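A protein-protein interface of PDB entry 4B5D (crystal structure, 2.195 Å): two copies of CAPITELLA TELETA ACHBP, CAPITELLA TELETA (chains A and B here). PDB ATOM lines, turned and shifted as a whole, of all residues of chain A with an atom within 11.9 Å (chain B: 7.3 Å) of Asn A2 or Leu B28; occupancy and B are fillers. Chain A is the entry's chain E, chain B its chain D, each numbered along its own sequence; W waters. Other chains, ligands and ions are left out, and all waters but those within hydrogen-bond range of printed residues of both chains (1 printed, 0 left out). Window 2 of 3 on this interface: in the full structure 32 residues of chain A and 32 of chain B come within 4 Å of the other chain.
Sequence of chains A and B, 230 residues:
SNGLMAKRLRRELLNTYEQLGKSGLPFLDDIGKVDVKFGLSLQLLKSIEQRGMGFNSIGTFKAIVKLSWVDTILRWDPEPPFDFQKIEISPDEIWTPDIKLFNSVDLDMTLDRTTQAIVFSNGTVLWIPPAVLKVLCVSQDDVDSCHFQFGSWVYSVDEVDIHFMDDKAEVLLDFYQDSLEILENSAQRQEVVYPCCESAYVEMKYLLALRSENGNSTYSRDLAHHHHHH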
ATOM      1  N   ASN A   2      33.907   9.124 -22.209  1.00  0.00           N
ATOM      2  CA  ASN A   2      33.461  10.466 -22.588  1.00  0.00           C
ATOM      3  C   ASN A   2      31.935  10.674 -22.459  1.00  0.00           C
ATOM      4  O   ASN A   2      31.141   9.841 -22.890  1.00  0.00           O
ATOM      5  CB  ASN A   2      33.900  10.765 -24.015  1.00  0.00           C
ATOM      6  CG  ASN A   2      33.339  12.074 -24.534  1.00  0.00           C
ATOM      7  OD1 ASN A   2      32.247  12.111 -25.107  1.00  0.00           O
ATOM      8  ND2 ASN A   2      34.086  13.156 -24.343  1.00  0.00           N
ATOM      9  N   GLY A   3      31.541  11.806 -21.882  1.00  0.00           N
ATOM     10  CA  GLY A   3      30.152  12.059 -21.542  1.00  0.00           C
ATOM     11  C   GLY A   3      29.234  12.188 -22.738  1.00  0.00           C
ATOM     12  O   GLY A   3      28.162  11.584 -22.767  1.00  0.00           O
ATOM     13  N   LEU A   4      29.654  12.980 -23.717  1.00  0.00           N
ATOM     14  CA  LEU A   4      28.930  13.127 -24.976  1.00  0.00           C
ATOM     15  C   LEU A   4      28.719  11.782 -25.660  1.00  0.00           C
ATOM     16  O   LEU A   4      27.602  11.455 -26.063  1.00  0.00           O
ATOM     17  CB  LEU A   4      29.690  14.049 -25.932  1.00  0.00           C
ATOM     18  CG  LEU A   4      28.954  14.356 -27.238  1.00  0.00           C
ATOM     19  CD1 LEU A   4      27.893  15.392 -26.977  1.00  0.00           C
ATOM     20  CD2 LEU A   4      29.907  14.828 -28.327  1.00  0.00           C
ATOM     21  N   MET A   5      29.796  11.005 -25.791  1.00  0.00           N
ATOM     22  CA  MET A   5      29.696   9.675 -26.391  1.00  0.00           C
ATOM     23  C   MET A   5      28.653   8.784 -25.702  1.00  0.00           C
ATOM     24  O   MET A   5      27.992   7.987 -26.353  1.00  0.00           O
ATOM     25  CB  MET A   5      31.062   8.994 -26.436  1.00  0.00           C
ATOM     26  CG  MET A   5      32.053   9.664 -27.404  1.00  0.00           C
ATOM     27  SD  MET A   5      31.520   9.587 -29.132  1.00  0.00           S
ATOM     28  CE  MET A   5      30.862  11.231 -29.386  1.00  0.00           C
ATOM     29  N   ALA A   6      28.498   8.933 -24.389  1.00  0.00           N
ATOM     30  CA  ALA A   6      27.484   8.185 -23.649  1.00  0.00           C
ATOM     31  C   ALA A   6      26.052   8.606 -24.021  1.00  0.00           C
ATOM     32  O   ALA A   6      25.167   7.758 -24.199  1.00  0.00           O
ATOM     33  CB  ALA A   6      27.713   8.319 -22.138  1.00  0.00           C
ATOM     34  N   LYS A   7      25.822   9.912 -24.129  1.00  0.00           N
ATOM     35  CA  LYS A   7      24.499  10.400 -24.494  1.00  0.00           C
ATOM     36  C   LYS A   7      24.184  10.011 -25.936  1.00  0.00           C
ATOM     37  O   LYS A   7      23.076   9.571 -26.221  1.00  0.00           O
ATOM     38  CB  LYS A   7      24.382  11.915 -24.306  1.00  0.00           C
ATOM     39  CG  LYS A   7      24.344  12.378 -22.851  1.00  0.00           C
ATOM     40  CD  LYS A   7      24.505  13.895 -22.757  1.00  0.00           C
ATOM     41  CE  LYS A   7      24.460  14.374 -21.309  1.00  0.00           C
ATOM     42  NZ  LYS A   7      23.166  14.041 -20.632  1.00  0.00           N
ATOM     43  N   ARG A   8      25.163  10.147 -26.833  1.00  0.00           N
ATOM     44  CA  ARG A   8      24.963   9.722 -28.216  1.00  0.00           C
ATOM     45  C   ARG A   8      24.661   8.226 -28.305  1.00  0.00           C
ATOM     46  O   ARG A   8      23.832   7.807 -29.113  1.00  0.00           O
ATOM     47  CB  ARG A   8      26.158  10.084 -29.113  1.00  0.00           C
ATOM     48  CG  ARG A   8      26.405  11.579 -29.231  1.00  0.00           C
ATOM     49  CD  ARG A   8      26.872  11.986 -30.622  1.00  0.00           C
ATOM     50  NE  ARG A   8      27.156  13.421 -30.705  1.00  0.00           N
ATOM     51  CZ  ARG A   8      26.252  14.363 -30.977  1.00  0.00           C
ATOM     52  NH1 ARG A   8      24.983  14.038 -31.203  1.00  0.00           N
ATOM     53  NH2 ARG A   8      26.620  15.640 -31.028  1.00  0.00           N
ATOM     54  N   LEU A   9      25.324   7.424 -27.473  1.00  0.00           N
ATOM     55  CA  LEU A   9      25.030   5.994 -27.434  1.00  0.00           C
ATOM     56  C   LEU A   9      23.564   5.752 -27.031  1.00  0.00           C
ATOM     57  O   LEU A   9      22.874   4.946 -27.650  1.00  0.00           O
ATOM     58  CB  LEU A   9      25.984   5.239 -26.496  1.00  0.00           C
ATOM     59  CG  LEU A   9      25.605   3.762 -26.269  1.00  0.00           C
ATOM     60  CD1 LEU A   9      25.684   2.991 -27.575  1.00  0.00           C
ATOM     61  CD2 LEU A   9      26.460   3.087 -25.185  1.00  0.00           C
ATOM     62  N   ARG A  10      23.096   6.463 -26.006  1.00  0.00           N
ATOM     63  CA  ARG A  10      21.715   6.335 -25.561  1.00  0.00           C
ATOM     64  C   ARG A  10      20.774   6.689 -26.710  1.00  0.00           C
ATOM     65  O   ARG A  10      19.856   5.929 -27.025  1.00  0.00           O
ATOM     66  CB  ARG A  10      21.432   7.211 -24.327  1.00  0.00           C
ATOM     67  CG  ARG A  10      19.992   7.082 -23.772  1.00  0.00           C
ATOM     68  CD  ARG A  10      19.778   7.890 -22.483  1.00  0.00           C
ATOM     69  NE  ARG A  10      20.673   7.480 -21.393  1.00  0.00           N
ATOM     70  CZ  ARG A  10      21.808   8.108 -21.083  1.00  0.00           C
ATOM     71  NH1 ARG A  10      22.177   9.173 -21.785  1.00  0.00           N
ATOM     72  NH2 ARG A  10      22.572   7.679 -20.072  1.00  0.00           N
ATOM     73  N   ARG A  11      21.032   7.818 -27.355  1.00  0.00           N
ATOM     74  CA  ARG A  11      20.209   8.239 -28.480  1.00  0.00           C
ATOM     75  C   ARG A  11      20.209   7.204 -29.599  1.00  0.00           C
ATOM     76  O   ARG A  11      19.159   6.937 -30.186  1.00  0.00           O
ATOM     77  CB  ARG A  11      20.641   9.618 -28.993  1.00  0.00           C
ATOM     78  CG  ARG A  11      20.349  10.755 -28.006  1.00  0.00           C
ATOM     79  CD  ARG A  11      18.935  11.350 -28.180  1.00  0.00           C
ATOM     80  NE  ARG A  11      17.855  10.439 -27.816  1.00  0.00           N
ATOM     81  CZ  ARG A  11      17.355  10.324 -26.586  1.00  0.00           C
ATOM     82  NH1 ARG A  11      17.855  11.053 -25.591  1.00  0.00           N
ATOM     83  NH2 ARG A  11      16.359   9.469 -26.340  1.00  0.00           N
ATOM     84  N   TRP A  76      24.783  -3.261 -27.499  1.00  0.00           N
ATOM     85  CA  TRP A  76      25.849  -2.631 -28.255  1.00  0.00           C
ATOM     86  C   TRP A  76      27.162  -3.345 -28.004  1.00  0.00           C
ATOM     87  O   TRP A  76      27.295  -4.111 -27.047  1.00  0.00           O
ATOM     88  CB  TRP A  76      25.969  -1.136 -27.939  1.00  0.00           C
ATOM     89  CG  TRP A  76      26.458  -0.807 -26.559  1.00  0.00           C
ATOM     90  CD1 TRP A  76      27.729  -0.450 -26.204  1.00  0.00           C
ATOM     91  CD2 TRP A  76      25.683  -0.785 -25.350  1.00  0.00           C
ATOM     92  NE1 TRP A  76      27.795  -0.212 -24.853  1.00  0.00           N
ATOM     93  CE2 TRP A  76      26.554  -0.413 -24.303  1.00  0.00           C
ATOM     94  CE3 TRP A  76      24.335  -1.050 -25.051  1.00  0.00           C
ATOM     95  CZ2 TRP A  76      26.125  -0.292 -22.973  1.00  0.00           C
ATOM     96  CZ3 TRP A  76      23.907  -0.930 -23.732  1.00  0.00           C
ATOM     97  CH2 TRP A  76      24.801  -0.553 -22.710  1.00  0.00           C
ATOM     98  N   PRO A  78      30.670  -2.828 -26.671  1.00  0.00           N
ATOM     99  CA  PRO A  78      31.351  -1.905 -25.767  1.00  0.00           C
ATOM    100  C   PRO A  78      32.824  -1.752 -26.125  1.00  0.00           C
ATOM    101  O   PRO A  78      33.702  -2.043 -25.312  1.00  0.00           O
ATOM    102  CB  PRO A  78      31.199  -2.590 -24.413  1.00  0.00           C
ATOM    103  CG  PRO A  78      31.182  -4.041 -24.750  1.00  0.00           C
ATOM    104  CD  PRO A  78      30.432  -4.140 -26.043  1.00  0.00           C
ATOM    105  N   GLU A  79      33.076  -1.311 -27.351  1.00  0.00           N
ATOM    106  CA  GLU A  79      34.413  -0.946 -27.802  1.00  0.00           C
ATOM    107  C   GLU A  79      34.361   0.531 -28.200  1.00  0.00           C
ATOM    108  O   GLU A  79      33.282   1.034 -28.538  1.00  0.00           O
ATOM    109  CB  GLU A  79      34.845  -1.839 -28.972  1.00  0.00           C
ATOM    110  CG  GLU A  79      33.837  -1.961 -30.109  1.00  0.00           C
ATOM    111  CD  GLU A  79      34.186  -3.091 -31.071  1.00  0.00           C
ATOM    112  OE1 GLU A  79      34.074  -4.275 -30.677  1.00  0.00           O
ATOM    113  OE2 GLU A  79      34.584  -2.792 -32.219  1.00  0.00           O
ATOM    114  N   PRO A  80      35.508   1.231 -28.137  1.00  0.00           N
ATOM    115  CA  PRO A  80      35.593   2.674 -28.412  1.00  0.00           C
ATOM    116  C   PRO A  80      34.905   3.065 -29.717  1.00  0.00           C
ATOM    117  O   PRO A  80      35.001   2.326 -30.700  1.00  0.00           O
ATOM    118  CB  PRO A  80      37.104   2.922 -28.552  1.00  0.00           C
ATOM    119  CG  PRO A  80      37.745   1.819 -27.842  1.00  0.00           C
ATOM    120  CD  PRO A  80      36.840   0.639 -27.898  1.00  0.00           C
ATOM    121  N   PRO A  81      34.226   4.224 -29.731  1.00  0.00           N
ATOM    122  CA  PRO A  81      34.115   5.139 -28.592  1.00  0.00           C
ATOM    123  C   PRO A  81      32.828   4.915 -27.791  1.00  0.00           C
ATOM    124  O   PRO A  81      32.338   5.852 -27.160  1.00  0.00           O
ATOM    125  CB  PRO A  81      34.063   6.501 -29.276  1.00  0.00           C
ATOM    126  CG  PRO A  81      33.273   6.217 -30.537  1.00  0.00           C
ATOM    127  CD  PRO A  81      33.591   4.788 -30.939  1.00  0.00           C
ATOM    128  N   PHE A  82      32.293   3.693 -27.827  1.00  0.00           N
ATOM    129  CA  PHE A  82      31.138   3.316 -27.021  1.00  0.00           C
ATOM    130  C   PHE A  82      31.484   2.265 -25.960  1.00  0.00           C
ATOM    131  O   PHE A  82      30.708   1.338 -25.692  1.00  0.00           O
ATOM    132  CB  PHE A  82      30.011   2.812 -27.920  1.00  0.00           C
ATOM    133  CG  PHE A  82      29.331   3.898 -28.695  1.00  0.00           C
ATOM    134  CD1 PHE A  82      29.427   5.219 -28.285  1.00  0.00           C
ATOM    135  CD2 PHE A  82      28.585   3.601 -29.825  1.00  0.00           C
ATOM    136  CE1 PHE A  82      28.798   6.222 -28.987  1.00  0.00           C
ATOM    137  CE2 PHE A  82      27.952   4.600 -30.534  1.00  0.00           C
ATOM    138  CZ  PHE A  82      28.063   5.915 -30.115  1.00  0.00           C
ATOM    139  N   ASP A  83      32.652   2.435 -25.352  1.00  0.00           N
ATOM    140  CA  ASP A  83      33.188   1.498 -24.376  1.00  0.00           C
ATOM    141  C   ASP A  83      32.575   1.717 -22.990  1.00  0.00           C
ATOM    142  O   ASP A  83      33.271   2.082 -22.037  1.00  0.00           O
ATOM    143  CB  ASP A  83      34.701   1.684 -24.311  1.00  0.00           C
ATOM    144  CG  ASP A  83      35.093   3.149 -24.265  1.00  0.00           C
ATOM    145  OD1 ASP A  83      35.098   3.798 -25.335  1.00  0.00           O
ATOM    146  OD2 ASP A  83      35.372   3.660 -23.158  1.00  0.00           O
ATOM    147  N   PHE A  84      31.266   1.513 -22.894  1.00  0.00           N
ATOM    148  CA  PHE A  84      30.556   1.625 -21.630  1.00  0.00           C
ATOM    149  C   PHE A  84      29.968   0.257 -21.319  1.00  0.00           C
ATOM    150  O   PHE A  84      29.429  -0.405 -22.210  1.00  0.00           O
ATOM    151  CB  PHE A  84      29.432   2.661 -21.718  1.00  0.00           C
ATOM    152  CG  PHE A  84      29.862   3.985 -22.289  1.00  0.00           C
ATOM    153  CD1 PHE A  84      30.375   4.984 -21.461  1.00  0.00           C
ATOM    154  CD2 PHE A  84      29.751   4.240 -23.651  1.00  0.00           C
ATOM    155  CE1 PHE A  84      30.780   6.208 -21.984  1.00  0.00           C
ATOM    156  CE2 PHE A  84      30.145   5.461 -24.176  1.00  0.00           C
ATOM    157  CZ  PHE A  84      30.667   6.446 -23.342  1.00  0.00           C
ATOM    158  N   GLN A  85      30.087  -0.173 -20.066  1.00  0.00           N
ATOM    159  CA  GLN A  85      29.558  -1.469 -19.651  1.00  0.00           C
ATOM    160  C   GLN A  85      28.048  -1.420 -19.443  1.00  0.00           C
ATOM    161  O   GLN A  85      27.356  -2.430 -19.568  1.00  0.00           O
ATOM    162  CB  GLN A  85      30.256  -1.949 -18.374  1.00  0.00           C
ATOM    163  CG  GLN A  85      31.694  -2.420 -18.610  1.00  0.00           C
ATOM    164  CD  GLN A  85      32.721  -1.630 -17.809  1.00  0.00           C
ATOM    165  OE1 GLN A  85      32.432  -0.543 -17.304  1.00  0.00           O
ATOM    166  NE2 GLN A  85      33.928  -2.178 -17.688  1.00  0.00           N
ATOM    167  N   LYS A  86      27.545  -0.237 -19.108  1.00  0.00           N
ATOM    168  CA  LYS A  86      26.131  -0.071 -18.809  1.00  0.00           C
ATOM    169  C   LYS A  86      25.739   1.384 -18.986  1.00  0.00           C
ATOM    170  O   LYS A  86      26.596   2.268 -19.004  1.00  0.00           O
ATOM    171  CB  LYS A  86      25.820  -0.530 -17.376  1.00  0.00           C
ATOM    172  CG  LYS A  86      26.670   0.156 -16.317  1.00  0.00           C
ATOM    173  CD  LYS A  86      26.378  -0.360 -14.915  1.00  0.00           C
ATOM    174  CE  LYS A  86      27.442   0.100 -13.910  1.00  0.00           C
ATOM    175  NZ  LYS A  86      27.571   1.585 -13.809  1.00  0.00           N
ATOM    176  N   ILE A  87      24.443   1.625 -19.115  1.00  0.00           N
ATOM    177  CA  ILE A  87      23.924   2.981 -19.248  1.00  0.00           C
ATOM    178  C   ILE A  87      22.555   3.079 -18.550  1.00  0.00           C
ATOM    179  O   ILE A  87      21.789   2.105 -18.527  1.00  0.00           O
ATOM    180  CB  ILE A  87      23.876   3.406 -20.749  1.00  0.00           C
ATOM    181  CG1 ILE A  87      24.133   4.899 -20.906  1.00  0.00           C
ATOM    182  CG2 ILE A  87      22.565   2.990 -21.445  1.00  0.00           C
ATOM    183  CD1 ILE A  87      24.260   5.328 -22.349  1.00  0.00           C
ATOM    184  N   GLU A  88      22.274   4.228 -17.938  1.00  0.00           N
ATOM    185  CA  GLU A  88      20.961   4.456 -17.330  1.00  0.00           C
ATOM    186  C   GLU A  88      19.964   4.953 -18.373  1.00  0.00           C
ATOM    187  O   GLU A  88      20.308   5.776 -19.222  1.00  0.00           O
ATOM    188  CB  GLU A  88      21.031   5.424 -16.144  1.00  0.00           C
ATOM    189  CG  GLU A  88      21.452   6.862 -16.482  1.00  0.00           C
ATOM    190  CD  GLU A  88      22.970   7.058 -16.552  1.00  0.00           C
ATOM    191  OE1 GLU A  88      23.647   6.297 -17.278  1.00  0.00           O
ATOM    192  OE2 GLU A  88      23.484   7.980 -15.878  1.00  0.00           O
ATOM    193  N   THR B  16      21.824  21.407 -25.589  1.00  0.00           N
ATOM    194  CA  THR B  16      22.438  20.102 -25.396  1.00  0.00           C
ATOM    195  C   THR B  16      21.432  19.104 -24.824  1.00  0.00           C
ATOM    196  O   THR B  16      21.223  18.025 -25.380  1.00  0.00           O
ATOM    197  CB  THR B  16      23.655  20.177 -24.441  1.00  0.00           C
ATOM    198  OG1 THR B  16      24.657  21.035 -24.997  1.00  0.00           O
ATOM    199  CG2 THR B  16      24.244  18.796 -24.226  1.00  0.00           C
ATOM    200  N   LEU B  20      20.145  15.630 -26.714  1.00  0.00           N
ATOM    201  CA  LEU B  20      20.703  14.362 -26.251  1.00  0.00           C
ATOM    202  C   LEU B  20      19.958  13.844 -25.040  1.00  0.00           C
ATOM    203  O   LEU B  20      20.256  12.763 -24.530  1.00  0.00           O
ATOM    204  CB  LEU B  20      22.173  14.517 -25.883  1.00  0.00           C
ATOM    205  CG  LEU B  20      23.128  15.034 -26.957  1.00  0.00           C
ATOM    206  CD1 LEU B  20      24.485  15.274 -26.340  1.00  0.00           C
ATOM    207  CD2 LEU B  20      23.233  14.057 -28.121  1.00  0.00           C
ATOM    208  N   LEU B  25      24.955  11.313 -16.282  1.00  0.00           N
ATOM    209  CA  LEU B  25      25.742  12.285 -15.534  1.00  0.00           C
ATOM    210  C   LEU B  25      26.089  13.518 -16.374  1.00  0.00           C
ATOM    211  O   LEU B  25      26.369  13.417 -17.568  1.00  0.00           O
ATOM    212  CB  LEU B  25      26.993  11.617 -14.950  1.00  0.00           C
ATOM    213  CG  LEU B  25      26.689  10.466 -13.982  1.00  0.00           C
ATOM    214  CD1 LEU B  25      27.981   9.787 -13.567  1.00  0.00           C
ATOM    215  CD2 LEU B  25      25.918  10.964 -12.755  1.00  0.00           C
ATOM    216  N   PRO B  26      26.034  14.696 -15.753  1.00  0.00           N
ATOM    217  CA  PRO B  26      26.135  15.955 -16.501  1.00  0.00           C
ATOM    218  C   PRO B  26      27.574  16.329 -16.856  1.00  0.00           C
ATOM    219  O   PRO B  26      28.116  17.269 -16.285  1.00  0.00           O
ATOM    220  CB  PRO B  26      25.535  16.975 -15.531  1.00  0.00           C
ATOM    221  CG  PRO B  26      25.881  16.425 -14.181  1.00  0.00           C
ATOM    222  CD  PRO B  26      25.786  14.918 -14.319  1.00  0.00           C
ATOM    223  N   PHE B  27      28.165  15.586 -17.791  1.00  0.00           N
ATOM    224  CA  PHE B  27      29.493  15.868 -18.331  1.00  0.00           C
ATOM    225  C   PHE B  27      29.453  15.594 -19.827  1.00  0.00           C
ATOM    226  O   PHE B  27      28.959  14.551 -20.260  1.00  0.00           O
ATOM    227  CB  PHE B  27      30.545  14.935 -17.722  1.00  0.00           C
ATOM    228  CG  PHE B  27      30.633  14.991 -16.226  1.00  0.00           C
ATOM    229  CD1 PHE B  27      29.789  14.203 -15.432  1.00  0.00           C
ATOM    230  CD2 PHE B  27      31.580  15.806 -15.606  1.00  0.00           C
ATOM    231  CE1 PHE B  27      29.867  14.253 -14.045  1.00  0.00           C
ATOM    232  CE2 PHE B  27      31.674  15.861 -14.219  1.00  0.00           C
ATOM    233  CZ  PHE B  27      30.812  15.087 -13.431  1.00  0.00           C
ATOM    234  N   LEU B  28      29.972  16.512 -20.625  1.00  0.00           N
ATOM    235  CA  LEU B  28      30.189  16.207 -22.034  1.00  0.00           C
ATOM    236  C   LEU B  28      31.570  15.580 -22.252  1.00  0.00           C
ATOM    237  O   LEU B  28      31.720  14.643 -23.042  1.00  0.00           O
ATOM    238  CB  LEU B  28      29.995  17.451 -22.912  1.00  0.00           C
ATOM    239  CG  LEU B  28      28.533  17.904 -23.099  1.00  0.00           C
ATOM    240  CD1 LEU B  28      28.439  19.099 -24.038  1.00  0.00           C
ATOM    241  CD2 LEU B  28      27.627  16.758 -23.578  1.00  0.00           C
ATOM    242  N   ASP B  29      32.574  16.084 -21.538  1.00  0.00           N
ATOM    243  CA  ASP B  29      33.939  15.587 -21.714  1.00  0.00           C
ATOM    244  C   ASP B  29      34.167  14.314 -20.901  1.00  0.00           C
ATOM    245  O   ASP B  29      33.396  13.358 -21.006  1.00  0.00           O
ATOM    246  CB  ASP B  29      34.959  16.671 -21.350  1.00  0.00           C
ATOM    247  CG  ASP B  29      34.895  17.867 -22.285  1.00  0.00           C
ATOM    248  OD1 ASP B  29      35.031  17.668 -23.513  1.00  0.00           O
ATOM    249  OD2 ASP B  29      34.688  19.001 -21.794  1.00  0.00           O
ATOM    250  N   ASP B  30      35.236  14.290 -20.110  1.00  0.00           N
ATOM    251  CA  ASP B  30      35.455  13.181 -19.198  1.00  0.00           C
ATOM    252  C   ASP B  30      34.286  13.072 -18.231  1.00  0.00           C
ATOM    253  O   ASP B  30      33.843  14.066 -17.664  1.00  0.00           O
ATOM    254  CB  ASP B  30      36.740  13.387 -18.404  1.00  0.00           C
ATOM    255  CG  ASP B  30      37.977  13.160 -19.231  1.00  0.00           C
ATOM    256  OD1 ASP B  30      37.847  12.961 -20.458  1.00  0.00           O
ATOM    257  OD2 ASP B  30      39.072  13.191 -18.636  1.00  0.00           O
ATOM    258  N   ILE B  31      33.783  11.865 -18.040  1.00  0.00           N
ATOM    259  CA  ILE B  31      32.746  11.679 -17.050  1.00  0.00           C
ATOM    260  C   ILE B  31      33.410  11.633 -15.688  1.00  0.00           C
ATOM    261  O   ILE B  31      34.282  10.797 -15.435  1.00  0.00           O
ATOM    262  CB  ILE B  31      31.919  10.417 -17.305  1.00  0.00           C
ATOM    263  CG1 ILE B  31      31.349  10.451 -18.724  1.00  0.00           C
ATOM    264  CG2 ILE B  31      30.797  10.326 -16.296  1.00  0.00           C
ATOM    265  CD1 ILE B  31      30.969   9.100 -19.276  1.00  0.00           C
ATOM    266  N   ASP B  71      26.995  21.404 -12.821  1.00  0.00           N
ATOM    267  CA  ASP B  71      26.623  20.784 -14.081  1.00  0.00           C
ATOM    268  C   ASP B  71      27.515  21.389 -15.150  1.00  0.00           C
ATOM    269  O   ASP B  71      27.397  22.566 -15.494  1.00  0.00           O
ATOM    270  CB  ASP B  71      25.128  20.970 -14.379  1.00  0.00           C
ATOM    271  CG  ASP B  71      24.690  20.324 -15.698  1.00  0.00           C
ATOM    272  OD1 ASP B  71      25.446  20.378 -16.702  1.00  0.00           O
ATOM    273  OD2 ASP B  71      23.560  19.780 -15.740  1.00  0.00           O
ATOM    274  N   THR B  72      28.400  20.542 -15.657  1.00  0.00           N
ATOM    275  CA  THR B  72      29.454  20.907 -16.587  1.00  0.00           C
ATOM    276  C   THR B  72      28.879  21.459 -17.881  1.00  0.00           C
ATOM    277  O   THR B  72      29.447  22.357 -18.505  1.00  0.00           O
ATOM    278  CB  THR B  72      30.338  19.660 -16.865  1.00  0.00           C
ATOM    279  OG1 THR B  72      31.479  19.697 -16.005  1.00  0.00           O
ATOM    280  CG2 THR B  72      30.772  19.569 -18.327  1.00  0.00           C
ATOM    281  N   ILE B  73      27.732  20.917 -18.263  1.00  0.00           N
ATOM    282  CA  ILE B  73      27.072  21.281 -19.508  1.00  0.00           C
ATOM    283  C   ILE B  73      26.484  22.702 -19.454  1.00  0.00           C
ATOM    284  O   ILE B  73      26.421  23.405 -20.467  1.00  0.00           O
ATOM    285  CB  ILE B  73      25.987  20.224 -19.868  1.00  0.00           C
ATOM    286  CG1 ILE B  73      26.625  18.828 -19.932  1.00  0.00           C
ATOM    287  CG2 ILE B  73      25.303  20.560 -21.177  1.00  0.00           C
ATOM    288  CD1 ILE B  73      25.701  17.727 -20.410  1.00  0.00           C
HETATM  289  O   HOH W   1      23.318  15.078 -17.958  1.00  0.00           O
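The backbone carbonyl oxygen (O) of Leu B20 lies within hydrogen-bond range of the guanidinium group (NH1) of Arg A11, 3.1 Å away.
The backbone carbonyl oxygen of Asp B29 lies close to the side-chain amide nitrogen of Asn A2 (3.4 Å).
N of Gly A3 is in hydrogen-bond range of O of Leu B28 (3.1 Å).
O of Leu B28 is in hydrogen-bond range of N of Leu A4 (2.7 Å).
O of Leu B28 sits at hydrogen-bond distance from ND2 of Asn A2 (3.1 Å).
The backbone carbonyl oxygen of Asp B29 lies within hydrogen-bond range of the backbone NH of Gly A3 (2.6 Å).
OD1 of Asn A2 is in hydrogen-bond range of N of Met A5 (2.8 Å).
N of Ile B73 sits at hydrogen-bond distance from OD1 of Asp B71.
NE1 of Trp A76 lies within hydrogen-bond range of O of Phe A84.
The guanidinium group (NH2) of Arg A10 is in salt-bridge range of the side-chain carboxylate (OE1) of Glu A88.
N of Leu A4 lies within hydrogen-bond range of OD1 of Asn A2.
Among the printed residues, merely in contact across the chains: Gly A3 with Phe B27 (3.0 Å), Gly A3 with Ile B31 (3.4 Å), Leu A4 with Leu B20 (3.5 Å), Arg A8 with Leu B20 (3.5 Å), Glu A88 with Leu B25 (3.7 Å), Asn A2 with Ile B31 (3.7 Å), Lys A7 with Ile B73 (3.7 Å), Lys A7 with Leu B20 (3.8 Å), Leu A4 with Phe B27 (3.9 Å) and Phe A84 with Ile B31 (3.97 Å).
Of the printed residues of chain B, Asn A2 touches Leu B28 (3.1 Å), Asp B29 (3.3 Å) and Ile B31 (3.7 Å).
No residue of chain A comes within 4 Å of Thr B16.
Printed residues of chain A within 4 Å of Leu B20: Leu A4, Lys A7, Arg A8 and Arg A11.
Of the printed residues of chain A, Leu B25 touches Glu A88 (3.7 Å).
No residue of chain A comes within 4 Å of Pro B26.
Of chain A, only Gly A3 (3.0 Å) and Leu A4 (3.9 Å) come within 4 Å of Phe B27.
Leu B28 touches three residues of chain A.
Asp B29 touches two residues of chain A.
No residue of chain A comes within 4 Å of Asp B30.
Ile B73 touches just one residue of chain A: Lys A7.
The nearest residue of chain B that does not touch Asn A2 is Asp B30 (4.5 Å).
Of the 22 printed residues of chain A, 8 touch a printed residue of chain B.
Hydrophobic or aromatic side chains of chain A within 4 Å of the printed part of chain B: Leu A4 and Phe A84.
Hydrophobic or aromatic side chains of chain B that line the printed part of chain A: Leu B20, Leu B28, Ile B31 and Ile B73.
Along chain B the printed residues that touch a printed residue of chain A span positions 20 to 73.
No position is printed for both chains.
Of the 16 pairs that touch across the chains among the printed residues, none has its exchanged pair printed and touching as well.
Water W1 lies within hydrogen-bond range of the side-chain amino group of Lys A7 (2.9 Å) and the backbone carbonyl oxygen of Leu B25 (3.5 Å).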
